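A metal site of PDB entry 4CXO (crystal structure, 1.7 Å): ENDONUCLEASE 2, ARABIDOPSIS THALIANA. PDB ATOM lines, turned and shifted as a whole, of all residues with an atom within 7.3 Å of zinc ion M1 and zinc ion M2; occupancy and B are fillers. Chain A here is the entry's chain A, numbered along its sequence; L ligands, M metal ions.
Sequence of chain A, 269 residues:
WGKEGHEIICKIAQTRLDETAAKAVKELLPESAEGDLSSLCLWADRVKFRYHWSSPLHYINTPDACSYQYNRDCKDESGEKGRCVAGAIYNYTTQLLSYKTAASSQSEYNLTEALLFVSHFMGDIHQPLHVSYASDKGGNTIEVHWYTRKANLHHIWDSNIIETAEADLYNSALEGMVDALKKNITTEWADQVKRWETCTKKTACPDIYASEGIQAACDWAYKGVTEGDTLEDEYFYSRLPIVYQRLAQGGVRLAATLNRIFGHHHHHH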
ATOM      1  N   TRP A   1     -23.447  14.469 -22.780  1.00  0.00           N
ATOM      2  CA  TRP A   1     -24.035  14.896 -24.064  1.00  0.00           C
ATOM      3  C   TRP A   1     -23.071  14.769 -25.197  1.00  0.00           C
ATOM      4  O   TRP A   1     -21.880  14.712 -24.993  1.00  0.00           O
ATOM      5  CB  TRP A   1     -24.445  16.363 -24.000  1.00  0.00           C
ATOM      6  CG  TRP A   1     -25.336  16.748 -22.851  1.00  0.00           C
ATOM      7  CD1 TRP A   1     -24.943  17.341 -21.696  1.00  0.00           C
ATOM      8  CD2 TRP A   1     -26.741  16.657 -22.801  1.00  0.00           C
ATOM      9  NE1 TRP A   1     -26.016  17.595 -20.900  1.00  0.00           N
ATOM     10  CE2 TRP A   1     -27.149  17.184 -21.549  1.00  0.00           C
ATOM     11  CE3 TRP A   1     -27.709  16.140 -23.662  1.00  0.00           C
ATOM     12  CZ2 TRP A   1     -28.482  17.223 -21.152  1.00  0.00           C
ATOM     13  CZ3 TRP A   1     -29.052  16.187 -23.276  1.00  0.00           C
ATOM     14  CH2 TRP A   1     -29.421  16.729 -22.022  1.00  0.00           C
ATOM     15  N   GLY A   2     -23.603  14.798 -26.410  1.00  0.00           N
ATOM     16  CA  GLY A   2     -22.782  14.878 -27.599  1.00  0.00           C
ATOM     17  C   GLY A   2     -22.376  16.309 -27.868  1.00  0.00           C
ATOM     18  O   GLY A   2     -22.596  17.198 -27.054  1.00  0.00           O
ATOM     19  N   LYS A   3     -21.788  16.539 -29.042  1.00  0.00           N
ATOM     20  CA  LYS A   3     -21.240  17.833 -29.408  1.00  0.00           C
ATOM     21  C   LYS A   3     -22.249  18.964 -29.303  1.00  0.00           C
ATOM     22  O   LYS A   3     -21.954  20.021 -28.762  1.00  0.00           O
ATOM     23  CB  LYS A   3     -20.712  17.757 -30.856  1.00  0.00           C
ATOM     24  CG  LYS A   3     -20.163  19.071 -31.427  1.00  0.00           C
ATOM     25  CD  LYS A   3     -19.690  18.907 -32.875  1.00  0.00           C
ATOM     26  CE  LYS A   3     -19.167  20.210 -33.455  1.00  0.00           C
ATOM     27  N   GLY A   5     -25.096  19.250 -27.601  1.00  0.00           N
ATOM     28  CA  GLY A   5     -25.493  19.562 -26.221  1.00  0.00           C
ATOM     29  C   GLY A   5     -24.476  20.404 -25.463  1.00  0.00           C
ATOM     30  O   GLY A   5     -24.848  21.393 -24.792  1.00  0.00           O
ATOM     31  N   HIS A   6     -23.215  20.020 -25.526  1.00  0.00           N
ATOM     32  CA  HIS A   6     -22.174  20.806 -24.878  1.00  0.00           C
ATOM     33  C   HIS A   6     -22.016  22.195 -25.477  1.00  0.00           C
ATOM     34  O   HIS A   6     -21.807  23.167 -24.774  1.00  0.00           O
ATOM     35  CB  HIS A   6     -20.832  20.059 -24.888  1.00  0.00           C
ATOM     36  CG  HIS A   6     -20.833  18.882 -23.989  1.00  0.00           C
ATOM     37  ND1 HIS A   6     -20.756  18.994 -22.618  1.00  0.00           N
ATOM     38  CD2 HIS A   6     -21.002  17.570 -24.258  1.00  0.00           C
ATOM     39  CE1 HIS A   6     -20.839  17.785 -22.091  1.00  0.00           C
ATOM     40  NE2 HIS A   6     -21.001  16.913 -23.067  1.00  0.00           N
ATOM     41  N   CYS A  41     -15.723  22.768 -25.441  1.00  0.00           N
ATOM     42  CA  CYS A  41     -16.544  22.105 -24.441  1.00  0.00           C
ATOM     43  C   CYS A  41     -16.723  20.610 -24.664  1.00  0.00           C
ATOM     44  O   CYS A  41     -17.321  19.950 -23.839  1.00  0.00           O
ATOM     45  CB  CYS A  41     -17.880  22.827 -24.245  1.00  0.00           C
ATOM     46  SG  CYS A  41     -17.639  24.281 -23.187  1.00  0.00           S
ATOM     47  N   LEU A  42     -16.175  20.084 -25.756  1.00  0.00           N
ATOM     48  CA  LEU A  42     -16.073  18.651 -25.951  1.00  0.00           C
ATOM     49  C   LEU A  42     -14.648  18.120 -25.679  1.00  0.00           C
ATOM     50  O   LEU A  42     -14.394  16.918 -25.792  1.00  0.00           O
ATOM     51  CB  LEU A  42     -16.523  18.265 -27.362  1.00  0.00           C
ATOM     52  CG  LEU A  42     -17.197  16.903 -27.532  1.00  0.00           C
ATOM     53  CD1 LEU A  42     -18.512  16.826 -26.766  1.00  0.00           C
ATOM     54  CD2 LEU A  42     -17.450  16.639 -29.008  1.00  0.00           C
ATOM     55  N   ALA A  44     -12.935  17.446 -23.050  1.00  0.00           N
ATOM     56  CA  ALA A  44     -12.869  16.358 -22.085  1.00  0.00           C
ATOM     57  C   ALA A  44     -13.202  15.008 -22.705  1.00  0.00           C
ATOM     58  O   ALA A  44     -12.620  13.991 -22.356  1.00  0.00           O
ATOM     59  CB  ALA A  44     -13.783  16.632 -20.901  1.00  0.00           C
ATOM     60  N   ASP A  45     -14.143  14.969 -23.643  1.00  0.00           N
ATOM     61  CA  ASP A  45     -14.452  13.698 -24.293  1.00  0.00           C
ATOM     62  C   ASP A  45     -13.286  13.216 -25.132  1.00  0.00           C
ATOM     63  O   ASP A  45     -13.155  12.027 -25.367  1.00  0.00           O
ATOM     64  CB  ASP A  45     -15.660  13.825 -25.200  1.00  0.00           C
ATOM     65  CG  ASP A  45     -16.953  13.580 -24.504  1.00  0.00           C
ATOM     66  OD1 ASP A  45     -16.961  13.244 -23.294  1.00  0.00           O
ATOM     67  OD2 ASP A  45     -17.974  13.732 -25.182  1.00  0.00           O
ATOM     68  N   LYS A  48     -10.573  10.981 -22.956  1.00  0.00           N
ATOM     69  CA  LYS A  48     -10.978   9.810 -22.207  1.00  0.00           C
ATOM     70  C   LYS A  48      -9.994   8.666 -22.288  1.00  0.00           C
ATOM     71  O   LYS A  48      -9.911   7.872 -21.356  1.00  0.00           O
ATOM     72  CB  LYS A  48     -12.332   9.278 -22.682  1.00  0.00           C
ATOM     73  CG  LYS A  48     -13.513  10.098 -22.251  1.00  0.00           C
ATOM     74  CD  LYS A  48     -14.780   9.469 -22.808  1.00  0.00           C
ATOM     75  CE  LYS A  48     -15.986  10.284 -22.436  1.00  0.00           C
ATOM     76  NZ  LYS A  48     -17.245   9.565 -22.695  1.00  0.00           N
ATOM     77  N   SER A  55     -12.103   8.770 -17.519  1.00  0.00           N
ATOM     78  CA  SER A  55     -13.293   8.227 -18.177  1.00  0.00           C
ATOM     79  C   SER A  55     -14.508   8.123 -17.234  1.00  0.00           C
ATOM     80  O   SER A  55     -15.615   8.525 -17.602  1.00  0.00           O
ATOM     81  CB  SER A  55     -12.973   6.872 -18.796  1.00  0.00           C
ATOM     82  OG  SER A  55     -14.105   6.354 -19.456  1.00  0.00           O
ATOM     83  N   LEU A  57     -15.168   9.898 -14.739  1.00  0.00           N
ATOM     84  CA  LEU A  57     -15.553  11.216 -14.258  1.00  0.00           C
ATOM     85  C   LEU A  57     -16.698  11.840 -15.062  1.00  0.00           C
ATOM     86  O   LEU A  57     -17.224  12.869 -14.693  1.00  0.00           O
ATOM     87  CB  LEU A  57     -14.334  12.152 -14.281  1.00  0.00           C
ATOM     88  CG  LEU A  57     -13.122  11.627 -13.525  1.00  0.00           C
ATOM     89  CD1 LEU A  57     -11.997  12.644 -13.565  1.00  0.00           C
ATOM     90  CD2 LEU A  57     -13.509  11.293 -12.082  1.00  0.00           C
ATOM     91  N   HIS A  58     -17.096  11.206 -16.153  1.00  0.00           N
ATOM     92  CA  HIS A  58     -18.181  11.769 -16.965  1.00  0.00           C
ATOM     93  C   HIS A  58     -19.564  11.428 -16.467  1.00  0.00           C
ATOM     94  O   HIS A  58     -20.548  12.015 -16.956  1.00  0.00           O
ATOM     95  CB  HIS A  58     -18.048  11.329 -18.413  1.00  0.00           C
ATOM     96  CG  HIS A  58     -16.851  11.914 -19.087  1.00  0.00           C
ATOM     97  ND1 HIS A  58     -16.969  12.831 -20.098  1.00  0.00           N
ATOM     98  CD2 HIS A  58     -15.530  11.747 -18.873  1.00  0.00           C
ATOM     99  CE1 HIS A  58     -15.763  13.197 -20.498  1.00  0.00           C
ATOM    100  NE2 HIS A  58     -14.874  12.548 -19.771  1.00  0.00           N
ATOM    101  N   TYR A  59     -19.662  10.512 -15.519  1.00  0.00           N
ATOM    102  CA  TYR A  59     -20.972   9.993 -15.132  1.00  0.00           C
ATOM    103  C   TYR A  59     -21.033   9.536 -13.676  1.00  0.00           C
ATOM    104  O   TYR A  59     -20.041   9.584 -12.944  1.00  0.00           O
ATOM    105  CB  TYR A  59     -21.387   8.858 -16.075  1.00  0.00           C
ATOM    106  CG  TYR A  59     -20.417   7.702 -16.099  1.00  0.00           C
ATOM    107  CD1 TYR A  59     -20.455   6.721 -15.118  1.00  0.00           C
ATOM    108  CD2 TYR A  59     -19.469   7.589 -17.097  1.00  0.00           C
ATOM    109  CE1 TYR A  59     -19.552   5.675 -15.105  1.00  0.00           C
ATOM    110  CE2 TYR A  59     -18.561   6.547 -17.103  1.00  0.00           C
ATOM    111  CZ  TYR A  59     -18.613   5.591 -16.110  1.00  0.00           C
ATOM    112  OH  TYR A  59     -17.724   4.563 -16.108  1.00  0.00           O
ATOM    113  N   HIS A 120     -17.232  20.954 -19.261  1.00  0.00           N
ATOM    114  CA  HIS A 120     -17.797  19.740 -19.815  1.00  0.00           C
ATOM    115  C   HIS A 120     -18.623  18.953 -18.788  1.00  0.00           C
ATOM    116  O   HIS A 120     -19.733  18.475 -19.078  1.00  0.00           O
ATOM    117  CB  HIS A 120     -16.681  18.846 -20.339  1.00  0.00           C
ATOM    118  CG  HIS A 120     -17.178  17.618 -21.016  1.00  0.00           C
ATOM    119  ND1 HIS A 120     -17.458  17.571 -22.361  1.00  0.00           N
ATOM    120  CD2 HIS A 120     -17.440  16.381 -20.528  1.00  0.00           C
ATOM    121  CE1 HIS A 120     -17.873  16.355 -22.681  1.00  0.00           C
ATOM    122  NE2 HIS A 120     -17.862  15.613 -21.588  1.00  0.00           N
ATOM    123  N   PHE A 121     -18.056  18.767 -17.597  1.00  0.00           N
ATOM    124  CA  PHE A 121     -18.715  17.994 -16.548  1.00  0.00           C
ATOM    125  C   PHE A 121     -19.991  18.658 -16.045  1.00  0.00           C
ATOM    126  O   PHE A 121     -20.976  17.969 -15.728  1.00  0.00           O
ATOM    127  CB  PHE A 121     -17.745  17.669 -15.423  1.00  0.00           C
ATOM    128  CG  PHE A 121     -16.618  16.749 -15.845  1.00  0.00           C
ATOM    129  CD1 PHE A 121     -16.830  15.729 -16.758  1.00  0.00           C
ATOM    130  CD2 PHE A 121     -15.353  16.900 -15.320  1.00  0.00           C
ATOM    131  CE1 PHE A 121     -15.799  14.885 -17.146  1.00  0.00           C
ATOM    132  CE2 PHE A 121     -14.322  16.056 -15.708  1.00  0.00           C
ATOM    133  CZ  PHE A 121     -14.539  15.045 -16.620  1.00  0.00           C
ATOM    134  N   GLY A 123     -21.938  20.180 -17.841  1.00  0.00           N
ATOM    135  CA  GLY A 123     -22.891  19.715 -18.844  1.00  0.00           C
ATOM    136  C   GLY A 123     -23.308  18.274 -18.633  1.00  0.00           C
ATOM    137  O   GLY A 123     -24.479  17.989 -18.585  1.00  0.00           O
ATOM    138  N   ASP A 124     -22.334  17.378 -18.500  1.00  0.00           N
ATOM    139  CA  ASP A 124     -22.632  15.950 -18.362  1.00  0.00           C
ATOM    140  C   ASP A 124     -23.487  15.604 -17.160  1.00  0.00           C
ATOM    141  O   ASP A 124     -24.359  14.740 -17.259  1.00  0.00           O
ATOM    142  CB  ASP A 124     -21.337  15.125 -18.336  1.00  0.00           C
ATOM    143  CG  ASP A 124     -20.871  14.756 -19.721  1.00  0.00           C
ATOM    144  OD1 ASP A 124     -21.533  15.155 -20.704  1.00  0.00           O
ATOM    145  OD2 ASP A 124     -19.838  14.058 -19.807  1.00  0.00           O
ATOM    146  N   ILE A 125     -23.301  16.310 -16.053  1.00  0.00           N
ATOM    147  CA  ILE A 125     -24.080  15.996 -14.848  1.00  0.00           C
ATOM    148  C   ILE A 125     -25.534  16.344 -15.048  1.00  0.00           C
ATOM    149  O   ILE A 125     -26.363  15.949 -14.248  1.00  0.00           O
ATOM    150  CB  ILE A 125     -23.512  16.674 -13.571  1.00  0.00           C
ATOM    151  CG1 ILE A 125     -24.039  15.972 -12.318  1.00  0.00           C
ATOM    152  CG2 ILE A 125     -23.817  18.156 -13.541  1.00  0.00           C
ATOM    153  CD1 ILE A 125     -23.269  16.290 -11.052  1.00  0.00           C
ATOM    154  N   GLN A 127     -27.106  15.572 -18.012  1.00  0.00           N
ATOM    155  CA  GLN A 127     -27.682  14.594 -18.931  1.00  0.00           C
ATOM    156  C   GLN A 127     -28.270  13.527 -18.017  1.00  0.00           C
ATOM    157  O   GLN A 127     -27.553  12.910 -17.252  1.00  0.00           O
ATOM    158  CB  GLN A 127     -26.603  14.039 -19.858  1.00  0.00           C
ATOM    159  CG  GLN A 127     -27.097  13.565 -21.234  1.00  0.00           C
ATOM    160  CD  GLN A 127     -27.798  12.207 -21.222  1.00  0.00           C
ATOM    161  OE1 GLN A 127     -28.788  12.026 -20.534  1.00  0.00           O
ATOM    162  NE2 GLN A 127     -27.307  11.281 -22.029  1.00  0.00           N
ATOM    163  N   HIS A 130     -26.569  10.239 -17.582  1.00  0.00           N
ATOM    164  CA  HIS A 130     -25.254  10.272 -16.964  1.00  0.00           C
ATOM    165  C   HIS A 130     -25.308  10.139 -15.442  1.00  0.00           C
ATOM    166  O   HIS A 130     -24.284  10.122 -14.799  1.00  0.00           O
ATOM    167  CB  HIS A 130     -24.518  11.560 -17.349  1.00  0.00           C
ATOM    168  CG  HIS A 130     -23.846  11.469 -18.670  1.00  0.00           C
ATOM    169  ND1 HIS A 130     -22.483  11.605 -18.816  1.00  0.00           N
ATOM    170  CD2 HIS A 130     -24.333  11.202 -19.899  1.00  0.00           C
ATOM    171  CE1 HIS A 130     -22.158  11.437 -20.080  1.00  0.00           C
ATOM    172  NE2 HIS A 130     -23.261  11.172 -20.756  1.00  0.00           N
ATOM    173  N   HIS A 154     -28.971   5.626 -24.313  1.00  0.00           N
ATOM    174  CA  HIS A 154     -28.035   6.649 -23.874  1.00  0.00           C
ATOM    175  C   HIS A 154     -27.722   7.653 -25.004  1.00  0.00           C
ATOM    176  O   HIS A 154     -27.755   8.874 -24.802  1.00  0.00           O
ATOM    177  CB  HIS A 154     -26.762   6.028 -23.332  1.00  0.00           C
ATOM    178  CG  HIS A 154     -25.811   7.024 -22.769  1.00  0.00           C
ATOM    179  ND1 HIS A 154     -25.771   7.340 -21.429  1.00  0.00           N
ATOM    180  CD2 HIS A 154     -24.945   7.854 -23.380  1.00  0.00           C
ATOM    181  CE1 HIS A 154     -24.875   8.293 -21.233  1.00  0.00           C
ATOM    182  NE2 HIS A 154     -24.360   8.622 -22.405  1.00  0.00           N
ATOM    183  N   ASP A 158     -27.894  11.622 -25.415  1.00  0.00           N
ATOM    184  CA  ASP A 158     -26.697  12.411 -25.713  1.00  0.00           C
ATOM    185  C   ASP A 158     -26.867  13.286 -26.965  1.00  0.00           C
ATOM    186  O   ASP A 158     -26.391  14.429 -26.990  1.00  0.00           O
ATOM    187  CB  ASP A 158     -25.481  11.510 -25.942  1.00  0.00           C
ATOM    188  CG  ASP A 158     -24.702  11.189 -24.685  1.00  0.00           C
ATOM    189  OD1 ASP A 158     -24.950  11.756 -23.596  1.00  0.00           O
ATOM    190  OD2 ASP A 158     -23.801  10.341 -24.802  1.00  0.00           O
HETATM  191  S1  LIG L   1     -20.263  12.261 -23.157  1.00  0.00           S
HETATM  192  O1  LIG L   1     -19.750  11.999 -24.540  1.00  0.00           O
HETATM  193  O2  LIG L   1     -19.432  11.452 -22.161  1.00  0.00           O
HETATM  194  O3  LIG L   1     -21.707  11.890 -23.202  1.00  0.00           O
HETATM  195  O4  LIG L   1     -20.061  13.724 -22.829  1.00  0.00           O
HETATM  196  P1  LG2 L   2     -18.832   3.987 -23.248  1.00  0.00           P
HETATM  197  O1  LG2 L   2     -17.633   3.966 -22.343  1.00  0.00           O
HETATM  198  O2  LG2 L   2     -18.492   4.138 -24.707  1.00  0.00           O
HETATM  199  O3  LG2 L   2     -19.888   2.941 -22.935  1.00  0.00           O
HETATM  200  O4  LG2 L   2     -19.573   5.373 -22.892  1.00  0.00           O
HETATM  201  C1  LG2 L   2     -20.648   5.790 -23.730  1.00  0.00           C
HETATM  202  C2  LG2 L   2     -21.427   6.925 -23.087  1.00  0.00           C
HETATM  203  O5  LG2 L   2     -22.133   6.535 -21.911  1.00  0.00           O
HETATM  204  C3  LG2 L   2     -20.550   8.048 -22.590  1.00  0.00           C
HETATM  205  O6  LG2 L   2     -21.356   9.206 -22.767  1.00  0.00           O
HETATM  206  C4  LG2 L   2     -20.312   7.803 -21.104  1.00  0.00           C
HETATM  207  C5  LG2 L   2     -21.674   7.219 -20.721  1.00  0.00           C
HETATM  208  N1  LG2 L   2     -21.750   6.223 -19.637  1.00  0.00           N
HETATM  209  C6  LG2 L   2     -22.699   6.407 -18.584  1.00  0.00           C
HETATM  210  O7  LG2 L   2     -23.414   7.441 -18.543  1.00  0.00           O
HETATM  211  N2  LG2 L   2     -22.826   5.487 -17.613  1.00  0.00           N
HETATM  212  C7  LG2 L   2     -22.087   4.383 -17.609  1.00  0.00           C
HETATM  213  O8  LG2 L   2     -22.229   3.550 -16.698  1.00  0.00           O
HETATM  214  C8  LG2 L   2     -21.096   4.155 -18.703  1.00  0.00           C
HETATM  215  C9  LG2 L   2     -20.234   2.936 -18.766  1.00  0.00           C
HETATM  216  C10 LG2 L   2     -20.989   5.112 -19.693  1.00  0.00           C
HETATM  217 ZN    ZN M   1     -18.524  13.494 -21.423  1.00  0.00          ZN
HETATM  218 ZN    ZN M   2     -21.463  14.975 -22.765  1.00  0.00          ZN
HETATM  219 ZN    ZN M   3     -23.113  10.342 -22.749  1.00  0.00          ZN
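The indole nitrogen (NE1) of Trp 1 lies within hydrogen-bond range of the backbone carbonyl oxygen (O) of Gly 123, at 2.8 Å. O of His 58 lies within hydrogen-bond range of ND1 of His 130, 2.7 Å away. The backbone carbonyl oxygen (O) of Cys 41 lies within hydrogen-bond range of a ring nitrogen (ND1) of His 120 (2.8 Å). The side-chain carboxylate (OD1) of Asp 45 sits close to the side-chain amino group (NZ) of Lys 48, at 3.7 Å.
Four residues have an atom within 4 Å of zinc ion M1: Asp 45, His 58, His 120 and Asp 124. The nearest printed residue that does not touch zinc ion M1 is Lys 48 (4.2 Å).
Of the 23 residues printed, 4 come within 4 Å of zinc ion M2. The nearest printed residue that does not touch zinc ion M2 is Gly 2 (4.2 Å).
Zinc ion M1 is bound by O4 of LIG L1. A ring nitrogen (ND1) of His 58 binds zinc ion M1 (2.1 Å). OD2 of Asp 124 is bound to zinc ion M1, 2.2 Å away. A ring nitrogen (NE2) of His 120 binds zinc ion M1 (2.2 Å). Zinc ion M1 is bound by an oxygen (O2) of LIG L1, 2.4 Å away. The side-chain carboxylate (OD1) of Asp 45 is bound to zinc ion M1 (2.5 Å). Zinc ion M1 has six donor atoms within binding distance.
Zinc ion M2 is bound by O4 of LIG L1, NE2 of His 6, N of Trp 1, OD1 of Asp 124 and O of Trp 1. Zinc ion M2 has five donor atoms within binding distance.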
